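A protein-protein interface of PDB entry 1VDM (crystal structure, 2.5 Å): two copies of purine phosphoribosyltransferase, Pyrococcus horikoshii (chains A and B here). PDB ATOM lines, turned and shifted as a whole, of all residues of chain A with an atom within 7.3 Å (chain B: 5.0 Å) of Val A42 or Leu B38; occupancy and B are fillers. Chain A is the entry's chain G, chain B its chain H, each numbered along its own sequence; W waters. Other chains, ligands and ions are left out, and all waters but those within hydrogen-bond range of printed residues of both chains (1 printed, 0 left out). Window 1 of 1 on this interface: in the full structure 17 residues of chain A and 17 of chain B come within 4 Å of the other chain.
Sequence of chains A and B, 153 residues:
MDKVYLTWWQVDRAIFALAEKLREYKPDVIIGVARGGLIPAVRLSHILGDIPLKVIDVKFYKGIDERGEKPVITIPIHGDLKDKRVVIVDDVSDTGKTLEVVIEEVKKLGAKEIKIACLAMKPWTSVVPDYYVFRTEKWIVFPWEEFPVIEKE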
ATOM      1  N   ILE A  15       5.879 -26.584  -9.441  1.00  0.00           N
ATOM      2  CA  ILE A  15       4.608 -26.025  -9.879  1.00  0.00           C
ATOM      3  C   ILE A  15       4.061 -25.045  -8.848  1.00  0.00           C
ATOM      4  O   ILE A  15       3.493 -24.021  -9.212  1.00  0.00           O
ATOM      5  CB  ILE A  15       3.565 -27.132 -10.117  1.00  0.00           C
ATOM      6  CG1 ILE A  15       3.939 -27.937 -11.355  1.00  0.00           C
ATOM      7  CG2 ILE A  15       2.175 -26.522 -10.289  1.00  0.00           C
ATOM      8  CD1 ILE A  15       2.976 -29.065 -11.638  1.00  0.00           C
ATOM      9  N   ILE A  30      -5.012 -20.368 -19.636  1.00  0.00           N
ATOM     10  CA  ILE A  30      -3.795 -21.157 -19.721  1.00  0.00           C
ATOM     11  C   ILE A  30      -3.808 -21.993 -20.991  1.00  0.00           C
ATOM     12  O   ILE A  30      -4.838 -22.545 -21.389  1.00  0.00           O
ATOM     13  CB  ILE A  30      -3.635 -22.130 -18.539  1.00  0.00           C
ATOM     14  CG1 ILE A  30      -3.488 -21.367 -17.226  1.00  0.00           C
ATOM     15  CG2 ILE A  30      -2.411 -22.992 -18.756  1.00  0.00           C
ATOM     16  CD1 ILE A  30      -3.352 -22.276 -16.007  1.00  0.00           C
ATOM     17  N   GLY A  32      -1.804 -25.135 -22.456  1.00  0.00           N
ATOM     18  CA  GLY A  32      -0.852 -26.191 -22.191  1.00  0.00           C
ATOM     19  C   GLY A  32      -0.347 -26.821 -23.469  1.00  0.00           C
ATOM     20  O   GLY A  32      -1.136 -27.198 -24.340  1.00  0.00           O
ATOM     21  N   ARG A  35       2.929 -32.980 -25.066  1.00  0.00           N
ATOM     22  CA  ARG A  35       2.043 -33.593 -24.085  1.00  0.00           C
ATOM     23  C   ARG A  35       2.506 -33.311 -22.654  1.00  0.00           C
ATOM     24  O   ARG A  35       1.723 -33.217 -21.718  1.00  0.00           O
ATOM     25  CB  ARG A  35       2.028 -35.102 -24.335  1.00  0.00           C
ATOM     26  CG  ARG A  35       1.796 -35.446 -25.806  1.00  0.00           C
ATOM     27  CD  ARG A  35       0.589 -36.372 -25.996  1.00  0.00           C
ATOM     28  NE  ARG A  35       0.018 -36.206 -27.335  1.00  0.00           N
ATOM     29  CZ  ARG A  35       0.394 -37.085 -28.281  1.00  0.00           C
ATOM     30  NH1 ARG A  35       1.246 -38.053 -27.986  1.00  0.00           N
ATOM     31  NH2 ARG A  35      -0.119 -36.993 -29.511  1.00  0.00           N
ATOM     32  N   GLY A  37       3.596 -30.697 -21.419  1.00  0.00           N
ATOM     33  CA  GLY A  37       3.062 -29.429 -20.935  1.00  0.00           C
ATOM     34  C   GLY A  37       1.810 -29.634 -20.077  1.00  0.00           C
ATOM     35  O   GLY A  37       1.516 -28.868 -19.170  1.00  0.00           O
ATOM     36  N   LEU A  38       0.945 -30.569 -20.456  1.00  0.00           N
ATOM     37  CA  LEU A  38      -0.357 -30.682 -19.817  1.00  0.00           C
ATOM     38  C   LEU A  38      -0.300 -31.044 -18.327  1.00  0.00           C
ATOM     39  O   LEU A  38      -1.270 -30.826 -17.605  1.00  0.00           O
ATOM     40  CB  LEU A  38      -1.242 -31.688 -20.573  1.00  0.00           C
ATOM     41  CG  LEU A  38      -1.632 -31.307 -22.011  1.00  0.00           C
ATOM     42  CD1 LEU A  38      -2.532 -32.379 -22.616  1.00  0.00           C
ATOM     43  CD2 LEU A  38      -2.340 -29.959 -22.019  1.00  0.00           C
ATOM     44  N   ILE A  39       0.816 -31.593 -17.854  1.00  0.00           N
ATOM     45  CA  ILE A  39       0.866 -31.913 -16.444  1.00  0.00           C
ATOM     46  C   ILE A  39       0.902 -30.634 -15.626  1.00  0.00           C
ATOM     47  O   ILE A  39       0.024 -30.356 -14.820  1.00  0.00           O
ATOM     48  CB  ILE A  39       2.128 -32.735 -16.183  1.00  0.00           C
ATOM     49  CG1 ILE A  39       1.833 -34.226 -16.362  1.00  0.00           C
ATOM     50  CG2 ILE A  39       2.602 -32.519 -14.735  1.00  0.00           C
ATOM     51  CD1 ILE A  39       1.687 -34.617 -17.834  1.00  0.00           C
ATOM     52  N   PRO A  40       1.920 -29.775 -15.834  1.00  0.00           N
ATOM     53  CA  PRO A  40       1.965 -28.519 -15.076  1.00  0.00           C
ATOM     54  C   PRO A  40       0.732 -27.653 -15.376  1.00  0.00           C
ATOM     55  O   PRO A  40       0.225 -26.956 -14.496  1.00  0.00           O
ATOM     56  CB  PRO A  40       3.253 -27.852 -15.568  1.00  0.00           C
ATOM     57  CG  PRO A  40       4.076 -28.992 -16.096  1.00  0.00           C
ATOM     58  CD  PRO A  40       3.046 -29.847 -16.781  1.00  0.00           C
ATOM     59  N   ALA A  41       0.262 -27.713 -16.621  1.00  0.00           N
ATOM     60  CA  ALA A  41      -0.893 -26.940 -17.065  1.00  0.00           C
ATOM     61  C   ALA A  41      -2.149 -27.236 -16.250  1.00  0.00           C
ATOM     62  O   ALA A  41      -2.767 -26.324 -15.706  1.00  0.00           O
ATOM     63  CB  ALA A  41      -1.160 -27.202 -18.538  1.00  0.00           C
ATOM     64  N   VAL A  42      -2.528 -28.510 -16.179  1.00  0.00           N
ATOM     65  CA  VAL A  42      -3.706 -28.919 -15.424  1.00  0.00           C
ATOM     66  C   VAL A  42      -3.576 -28.473 -13.970  1.00  0.00           C
ATOM     67  O   VAL A  42      -4.491 -27.866 -13.425  1.00  0.00           O
ATOM     68  CB  VAL A  42      -3.914 -30.465 -15.483  1.00  0.00           C
ATOM     69  CG1 VAL A  42      -4.869 -30.920 -14.394  1.00  0.00           C
ATOM     70  CG2 VAL A  42      -4.480 -30.846 -16.836  1.00  0.00           C
ATOM     71  N   ARG A  43      -2.437 -28.770 -13.354  1.00  0.00           N
ATOM     72  CA  ARG A  43      -2.201 -28.385 -11.973  1.00  0.00           C
ATOM     73  C   ARG A  43      -2.320 -26.869 -11.778  1.00  0.00           C
ATOM     74  O   ARG A  43      -2.959 -26.416 -10.824  1.00  0.00           O
ATOM     75  CB  ARG A  43      -0.830 -28.879 -11.514  1.00  0.00           C
ATOM     76  CG  ARG A  43      -0.805 -30.351 -11.123  1.00  0.00           C
ATOM     77  CD  ARG A  43      -0.331 -30.506  -9.683  1.00  0.00           C
ATOM     78  NE  ARG A  43      -1.113 -29.641  -8.800  1.00  0.00           N
ATOM     79  CZ  ARG A  43      -0.740 -29.279  -7.581  1.00  0.00           C
ATOM     80  NH1 ARG A  43       0.409 -29.710  -7.085  1.00  0.00           N
ATOM     81  NH2 ARG A  43      -1.509 -28.469  -6.866  1.00  0.00           N
ATOM     82  N   LEU A  44      -1.728 -26.088 -12.680  1.00  0.00           N
ATOM     83  CA  LEU A  44      -1.807 -24.632 -12.573  1.00  0.00           C
ATOM     84  C   LEU A  44      -3.241 -24.135 -12.787  1.00  0.00           C
ATOM     85  O   LEU A  44      -3.649 -23.119 -12.216  1.00  0.00           O
ATOM     86  CB  LEU A  44      -0.863 -23.961 -13.581  1.00  0.00           C
ATOM     87  CG  LEU A  44       0.638 -24.000 -13.268  1.00  0.00           C
ATOM     88  CD1 LEU A  44       1.420 -23.434 -14.454  1.00  0.00           C
ATOM     89  CD2 LEU A  44       0.938 -23.206 -12.003  1.00  0.00           C
ATOM     90  N   SER A  45      -4.004 -24.846 -13.611  1.00  0.00           N
ATOM     91  CA  SER A  45      -5.392 -24.464 -13.857  1.00  0.00           C
ATOM     92  C   SER A  45      -6.177 -24.532 -12.543  1.00  0.00           C
ATOM     93  O   SER A  45      -7.003 -23.667 -12.261  1.00  0.00           O
ATOM     94  CB  SER A  45      -6.035 -25.398 -14.878  1.00  0.00           C
ATOM     95  OG  SER A  45      -7.378 -25.020 -15.112  1.00  0.00           O
ATOM     96  N   HIS A  46      -5.906 -25.567 -11.752  1.00  0.00           N
ATOM     97  CA  HIS A  46      -6.555 -25.771 -10.462  1.00  0.00           C
ATOM     98  C   HIS A  46      -6.037 -24.780  -9.415  1.00  0.00           C
ATOM     99  O   HIS A  46      -6.819 -24.057  -8.804  1.00  0.00           O
ATOM    100  CB  HIS A  46      -6.307 -27.206  -9.967  1.00  0.00           C
ATOM    101  CG  HIS A  46      -7.101 -28.248 -10.693  1.00  0.00           C
ATOM    102  ND1 HIS A  46      -8.438 -28.474 -10.442  1.00  0.00           N
ATOM    103  CD2 HIS A  46      -6.748 -29.129 -11.661  1.00  0.00           C
ATOM    104  CE1 HIS A  46      -8.873 -29.449 -11.222  1.00  0.00           C
ATOM    105  NE2 HIS A  46      -7.868 -29.863 -11.971  1.00  0.00           N
ATOM    106  N   ILE A  47      -4.718 -24.744  -9.225  1.00  0.00           N
ATOM    107  CA  ILE A  47      -4.076 -23.865  -8.249  1.00  0.00           C
ATOM    108  C   ILE A  47      -4.370 -22.373  -8.410  1.00  0.00           C
ATOM    109  O   ILE A  47      -4.308 -21.622  -7.440  1.00  0.00           O
ATOM    110  CB  ILE A  47      -2.543 -24.034  -8.266  1.00  0.00           C
ATOM    111  CG1 ILE A  47      -2.170 -25.502  -8.076  1.00  0.00           C
ATOM    112  CG2 ILE A  47      -1.920 -23.214  -7.146  1.00  0.00           C
ATOM    113  CD1 ILE A  47      -0.675 -25.747  -8.033  1.00  0.00           C
ATOM    114  N   LEU A  48      -4.686 -21.938  -9.622  1.00  0.00           N
ATOM    115  CA  LEU A  48      -4.956 -20.525  -9.852  1.00  0.00           C
ATOM    116  C   LEU A  48      -6.439 -20.155  -9.946  1.00  0.00           C
ATOM    117  O   LEU A  48      -6.795 -19.176 -10.608  1.00  0.00           O
ATOM    118  CB  LEU A  48      -4.232 -20.061 -11.117  1.00  0.00           C
ATOM    119  CG  LEU A  48      -2.702 -20.108 -11.087  1.00  0.00           C
ATOM    120  CD1 LEU A  48      -2.170 -19.715 -12.452  1.00  0.00           C
ATOM    121  CD2 LEU A  48      -2.163 -19.171 -10.017  1.00  0.00           C
ATOM    122  N   ASP A  50      -9.263 -22.413 -10.867  1.00  0.00           N
ATOM    123  CA  ASP A  50      -9.915 -23.044 -12.010  1.00  0.00           C
ATOM    124  C   ASP A  50     -10.079 -22.143 -13.226  1.00  0.00           C
ATOM    125  O   ASP A  50     -11.173 -22.041 -13.780  1.00  0.00           O
ATOM    126  CB  ASP A  50     -11.288 -23.600 -11.610  1.00  0.00           C
ATOM    127  CG  ASP A  50     -11.191 -24.902 -10.825  1.00  0.00           C
ATOM    128  OD1 ASP A  50     -12.253 -25.482 -10.502  1.00  0.00           O
ATOM    129  OD2 ASP A  50     -10.058 -25.347 -10.530  1.00  0.00           O
ATOM    130  N   ILE A  51      -8.999 -21.487 -13.640  1.00  0.00           N
ATOM    131  CA  ILE A  51      -9.063 -20.629 -14.816  1.00  0.00           C
ATOM    132  C   ILE A  51      -9.060 -21.553 -16.030  1.00  0.00           C
ATOM    133  O   ILE A  51      -8.373 -22.577 -16.042  1.00  0.00           O
ATOM    134  CB  ILE A  51      -7.857 -19.668 -14.897  1.00  0.00           C
ATOM    135  CG1 ILE A  51      -6.559 -20.469 -14.946  1.00  0.00           C
ATOM    136  CG2 ILE A  51      -7.870 -18.702 -13.706  1.00  0.00           C
ATOM    137  CD1 ILE A  51      -5.334 -19.607 -15.054  1.00  0.00           C
ATOM    138  N   LEU A  53      -8.655 -23.787 -19.338  1.00  0.00           N
ATOM    139  CA  LEU A  53      -7.481 -24.438 -19.899  1.00  0.00           C
ATOM    140  C   LEU A  53      -7.674 -24.794 -21.370  1.00  0.00           C
ATOM    141  O   LEU A  53      -8.626 -25.488 -21.734  1.00  0.00           O
ATOM    142  CB  LEU A  53      -7.156 -25.715 -19.125  1.00  0.00           C
ATOM    143  CG  LEU A  53      -5.978 -26.524 -19.674  1.00  0.00           C
ATOM    144  CD1 LEU A  53      -4.692 -25.739 -19.481  1.00  0.00           C
ATOM    145  CD2 LEU A  53      -5.884 -27.856 -18.966  1.00  0.00           C
ATOM    146  N   LYS A  54      -6.770 -24.304 -22.210  1.00  0.00           N
ATOM    147  CA  LYS A  54      -6.821 -24.604 -23.632  1.00  0.00           C
ATOM    148  C   LYS A  54      -5.639 -25.512 -23.970  1.00  0.00           C
ATOM    149  O   LYS A  54      -4.540 -25.338 -23.438  1.00  0.00           O
ATOM    150  CB  LYS A  54      -6.777 -23.314 -24.454  1.00  0.00           C
ATOM    151  CG  LYS A  54      -8.100 -22.568 -24.444  1.00  0.00           C
ATOM    152  CD  LYS A  54      -8.079 -21.336 -25.330  1.00  0.00           C
ATOM    153  CE  LYS A  54      -9.456 -20.680 -25.382  1.00  0.00           C
ATOM    154  NZ  LYS A  54     -10.500 -21.601 -25.921  1.00  0.00           N
ATOM    155  N   VAL A  55      -5.871 -26.497 -24.829  1.00  0.00           N
ATOM    156  CA  VAL A  55      -4.811 -27.418 -25.198  1.00  0.00           C
ATOM    157  C   VAL A  55      -4.360 -27.290 -26.647  1.00  0.00           C
ATOM    158  O   VAL A  55      -5.176 -27.185 -27.568  1.00  0.00           O
ATOM    159  CB  VAL A  55      -5.238 -28.873 -24.946  1.00  0.00           C
ATOM    160  CG1 VAL A  55      -4.158 -29.826 -25.429  1.00  0.00           C
ATOM    161  CG2 VAL A  55      -5.493 -29.079 -23.464  1.00  0.00           C
ATOM    162  N   VAL A  89       1.998 -22.828 -20.781  1.00  0.00           N
ATOM    163  CA  VAL A  89       2.665 -23.761 -19.886  1.00  0.00           C
ATOM    164  C   VAL A  89       3.207 -24.954 -20.645  1.00  0.00           C
ATOM    165  O   VAL A  89       2.493 -25.594 -21.414  1.00  0.00           O
ATOM    166  CB  VAL A  89       1.704 -24.263 -18.790  1.00  0.00           C
ATOM    167  CG1 VAL A  89       2.457 -25.134 -17.793  1.00  0.00           C
ATOM    168  CG2 VAL A  89       1.061 -23.075 -18.092  1.00  0.00           C
ATOM    169  N   GLY B  32      -9.210 -37.906 -24.522  1.00  0.00           N
ATOM    170  CA  GLY B  32      -9.111 -37.562 -23.112  1.00  0.00           C
ATOM    171  C   GLY B  32     -10.077 -36.462 -22.713  1.00  0.00           C
ATOM    172  O   GLY B  32     -10.109 -35.396 -23.336  1.00  0.00           O
ATOM    173  N   VAL B  33     -10.877 -36.726 -21.682  1.00  0.00           N
ATOM    174  CA  VAL B  33     -11.758 -35.706 -21.134  1.00  0.00           C
ATOM    175  C   VAL B  33     -11.017 -34.661 -20.302  1.00  0.00           C
ATOM    176  O   VAL B  33     -10.328 -34.951 -19.335  1.00  0.00           O
ATOM    177  CB  VAL B  33     -12.804 -36.399 -20.261  1.00  0.00           C
ATOM    178  CG1 VAL B  33     -13.728 -35.353 -19.636  1.00  0.00           C
ATOM    179  CG2 VAL B  33     -13.628 -37.346 -21.114  1.00  0.00           C
ATOM    180  N   ALA B  34     -11.144 -33.398 -20.736  1.00  0.00           N
ATOM    181  CA  ALA B  34     -10.651 -32.316 -19.900  1.00  0.00           C
ATOM    182  C   ALA B  34     -11.546 -32.163 -18.663  1.00  0.00           C
ATOM    183  O   ALA B  34     -12.766 -32.256 -18.740  1.00  0.00           O
ATOM    184  CB  ALA B  34     -10.673 -31.028 -20.726  1.00  0.00           C
ATOM    185  N   ARG B  35     -10.912 -31.972 -17.482  1.00  0.00           N
ATOM    186  CA  ARG B  35      -9.455 -31.856 -17.415  1.00  0.00           C
ATOM    187  C   ARG B  35      -8.838 -33.091 -16.740  1.00  0.00           C
ATOM    188  O   ARG B  35      -7.654 -33.392 -16.870  1.00  0.00           O
ATOM    189  CB  ARG B  35      -9.137 -30.623 -16.571  1.00  0.00           C
ATOM    190  CG  ARG B  35      -9.249 -29.314 -17.353  1.00  0.00           C
ATOM    191  CD  ARG B  35      -9.208 -28.097 -16.414  1.00  0.00           C
ATOM    192  NE  ARG B  35     -10.283 -28.174 -15.414  1.00  0.00           N
ATOM    193  CZ  ARG B  35     -10.084 -27.552 -14.231  1.00  0.00           C
ATOM    194  NH1 ARG B  35      -8.946 -26.923 -13.995  1.00  0.00           N
ATOM    195  NH2 ARG B  35     -11.054 -27.550 -13.306  1.00  0.00           N
ATOM    196  N   GLY B  36      -9.689 -33.789 -15.963  1.00  0.00           N
ATOM    197  CA  GLY B  36      -9.204 -34.900 -15.155  1.00  0.00           C
ATOM    198  C   GLY B  36      -8.708 -36.061 -16.018  1.00  0.00           C
ATOM    199  O   GLY B  36      -8.010 -36.958 -15.562  1.00  0.00           O
ATOM    200  N   GLY B  37      -9.133 -36.046 -17.297  1.00  0.00           N
ATOM    201  CA  GLY B  37      -8.750 -37.127 -18.199  1.00  0.00           C
ATOM    202  C   GLY B  37      -7.354 -36.908 -18.787  1.00  0.00           C
ATOM    203  O   GLY B  37      -6.623 -37.849 -19.067  1.00  0.00           O
ATOM    204  N   LEU B  38      -6.989 -35.647 -19.009  1.00  0.00           N
ATOM    205  CA  LEU B  38      -5.728 -35.281 -19.642  1.00  0.00           C
ATOM    206  C   LEU B  38      -4.449 -35.980 -19.197  1.00  0.00           C
ATOM    207  O   LEU B  38      -3.774 -36.596 -20.018  1.00  0.00           O
ATOM    208  CB  LEU B  38      -5.513 -33.774 -19.544  1.00  0.00           C
ATOM    209  CG  LEU B  38      -6.600 -32.934 -20.204  1.00  0.00           C
ATOM    210  CD1 LEU B  38      -6.255 -31.459 -20.064  1.00  0.00           C
ATOM    211  CD2 LEU B  38      -6.737 -33.326 -21.664  1.00  0.00           C
ATOM    212  N   ILE B  39      -4.085 -35.884 -17.925  1.00  0.00           N
ATOM    213  CA  ILE B  39      -2.847 -36.522 -17.511  1.00  0.00           C
ATOM    214  C   ILE B  39      -2.816 -38.013 -17.835  1.00  0.00           C
ATOM    215  O   ILE B  39      -1.838 -38.496 -18.408  1.00  0.00           O
ATOM    216  CB  ILE B  39      -2.544 -36.277 -16.024  1.00  0.00           C
ATOM    217  CG1 ILE B  39      -2.154 -34.806 -15.838  1.00  0.00           C
ATOM    218  CG2 ILE B  39      -1.420 -37.202 -15.548  1.00  0.00           C
ATOM    219  CD1 ILE B  39      -1.581 -34.475 -14.475  1.00  0.00           C
ATOM    220  N   PRO B  40      -3.877 -38.765 -17.479  1.00  0.00           N
ATOM    221  CA  PRO B  40      -3.903 -40.203 -17.774  1.00  0.00           C
ATOM    222  C   PRO B  40      -3.790 -40.479 -19.278  1.00  0.00           C
ATOM    223  O   PRO B  40      -3.024 -41.340 -19.700  1.00  0.00           O
ATOM    224  CB  PRO B  40      -5.249 -40.644 -17.202  1.00  0.00           C
ATOM    225  CG  PRO B  40      -5.404 -39.740 -16.027  1.00  0.00           C
ATOM    226  CD  PRO B  40      -5.007 -38.401 -16.606  1.00  0.00           C
ATOM    227  N   ALA B  41      -4.556 -39.735 -20.075  1.00  0.00           N
ATOM    228  CA  ALA B  41      -4.546 -39.880 -21.529  1.00  0.00           C
ATOM    229  C   ALA B  41      -3.148 -39.649 -22.128  1.00  0.00           C
ATOM    230  O   ALA B  41      -2.741 -40.346 -23.056  1.00  0.00           O
ATOM    231  CB  ALA B  41      -5.543 -38.916 -22.149  1.00  0.00           C
ATOM    232  N   VAL B  42      -2.421 -38.670 -21.604  1.00  0.00           N
ATOM    233  CA  VAL B  42      -1.076 -38.380 -22.083  1.00  0.00           C
ATOM    234  C   VAL B  42      -0.187 -39.603 -21.904  1.00  0.00           C
ATOM    235  O   VAL B  42       0.482 -40.031 -22.840  1.00  0.00           O
ATOM    236  CB  VAL B  42      -0.462 -37.172 -21.322  1.00  0.00           C
ATOM    237  CG1 VAL B  42       1.061 -37.249 -21.325  1.00  0.00           C
ATOM    238  CG2 VAL B  42      -0.912 -35.877 -21.977  1.00  0.00           C
ATOM    239  N   VAL B  55      -8.661 -34.178 -27.620  1.00  0.00           N
ATOM    240  CA  VAL B  55      -9.194 -33.637 -26.373  1.00  0.00           C
ATOM    241  C   VAL B  55     -10.620 -33.116 -26.517  1.00  0.00           C
ATOM    242  O   VAL B  55     -11.031 -32.668 -27.588  1.00  0.00           O
ATOM    243  CB  VAL B  55      -8.283 -32.503 -25.833  1.00  0.00           C
ATOM    244  CG1 VAL B  55      -8.959 -31.777 -24.687  1.00  0.00           C
ATOM    245  CG2 VAL B  55      -6.967 -33.091 -25.354  1.00  0.00           C
ATOM    246  N   TRP B 144      -3.555 -34.188  -9.171  1.00  0.00           N
ATOM    247  CA  TRP B 144      -3.489 -32.916  -9.863  1.00  0.00           C
ATOM    248  C   TRP B 144      -4.462 -31.895  -9.309  1.00  0.00           C
ATOM    249  O   TRP B 144      -4.362 -30.706  -9.608  1.00  0.00           O
ATOM    250  CB  TRP B 144      -3.704 -33.113 -11.362  1.00  0.00           C
ATOM    251  CG  TRP B 144      -4.797 -34.054 -11.727  1.00  0.00           C
ATOM    252  CD1 TRP B 144      -6.085 -33.734 -12.044  1.00  0.00           C
ATOM    253  CD2 TRP B 144      -4.681 -35.474 -11.893  1.00  0.00           C
ATOM    254  NE1 TRP B 144      -6.776 -34.867 -12.408  1.00  0.00           N
ATOM    255  CE2 TRP B 144      -5.938 -35.948 -12.320  1.00  0.00           C
ATOM    256  CE3 TRP B 144      -3.634 -36.392 -11.724  1.00  0.00           C
ATOM    257  CZ2 TRP B 144      -6.177 -37.299 -12.580  1.00  0.00           C
ATOM    258  CZ3 TRP B 144      -3.874 -37.744 -11.984  1.00  0.00           C
ATOM    259  CH2 TRP B 144      -5.136 -38.180 -12.407  1.00  0.00           C
HETATM  260  O   HOH W   1      -9.529 -32.316 -12.901  1.00  0.00           O
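CG2 of Val B42 touches O of Arg A35 (3.8 Å).
Val B42 touches Leu A38.
Ile A39 touches Ile B39 (CG1 to CD1, 3.9 Å).
Leu B38 touches Val A42.
Trp B144 touches Val A42.
O of Trp B144 touches NE of Arg A43, at 3.5 Å.
Arg B35 touches His A46.
His A46 touches Trp B144 (CD2 to O, 3.5 Å).
Leu A53 touches Leu B38 (CD2 to CD1, 3.8 Å).
Arg A35 touches Val B42, but with the chains exchanged Val A42 does not touch Arg B35 (4.1 Å).
Leu A38 touches Val B42, and with the chains exchanged Val A42 touches Leu B38.
Ile A39 touches its own counterpart, Ile B39.
9 positions are printed for both chains.
OG of Ser A45 lies within hydrogen-bond range of NH1 of Arg B35, 2.7 Å away.
OD2 of Asp A50 lies within salt-bridge range of NH2 of Arg B35.
Printed residues of chain A that touch a printed residue of chain B: Arg A35, Leu A38, Ile A39, Val A42, Arg A43, Ser A45, His A46, Asp A50 and Leu A53.
Hydrophobic or aromatic side chains of chain B that line the printed part of chain A: Leu B38, Ile B39, Val B42 and Trp B144.
Among the printed residues, 11 pairs touch across the chains.
Water W1 bridges NE2 of His A46 (3.1 Å) and N of Gly B36 (3.4 Å).
Val A42 touches just these residues of chain B: Leu B38 and Trp B144.
Of chain A, only Val A42 and Leu A53 come within 4 Å of Leu B38.
No residue of chain A comes within 4 Å of Gly B37.
Of the printed residues of chain B, Leu A38 touches Val B42.
Of the printed residues of chain B, His A46 touches Arg B35 (3.6 Å) and Trp B144 (3.5 Å).
Printed residues of chain B within 4 Å of Leu A53: Leu B38.
Ile A15 touches none of the printed residues of chain B.
O of Ser A45 is in hydrogen-bond range of N of Asp A50 (2.9 Å).
The side-chain hydroxyl of Ser A45 lies within hydrogen-bond range of the backbone carbonyl oxygen of Ile A51 (2.8 Å).
The backbone NH (N) of Leu B38 is in hydrogen-bond range of the backbone carbonyl oxygen (O) of Val B33, 3.4 Å away.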
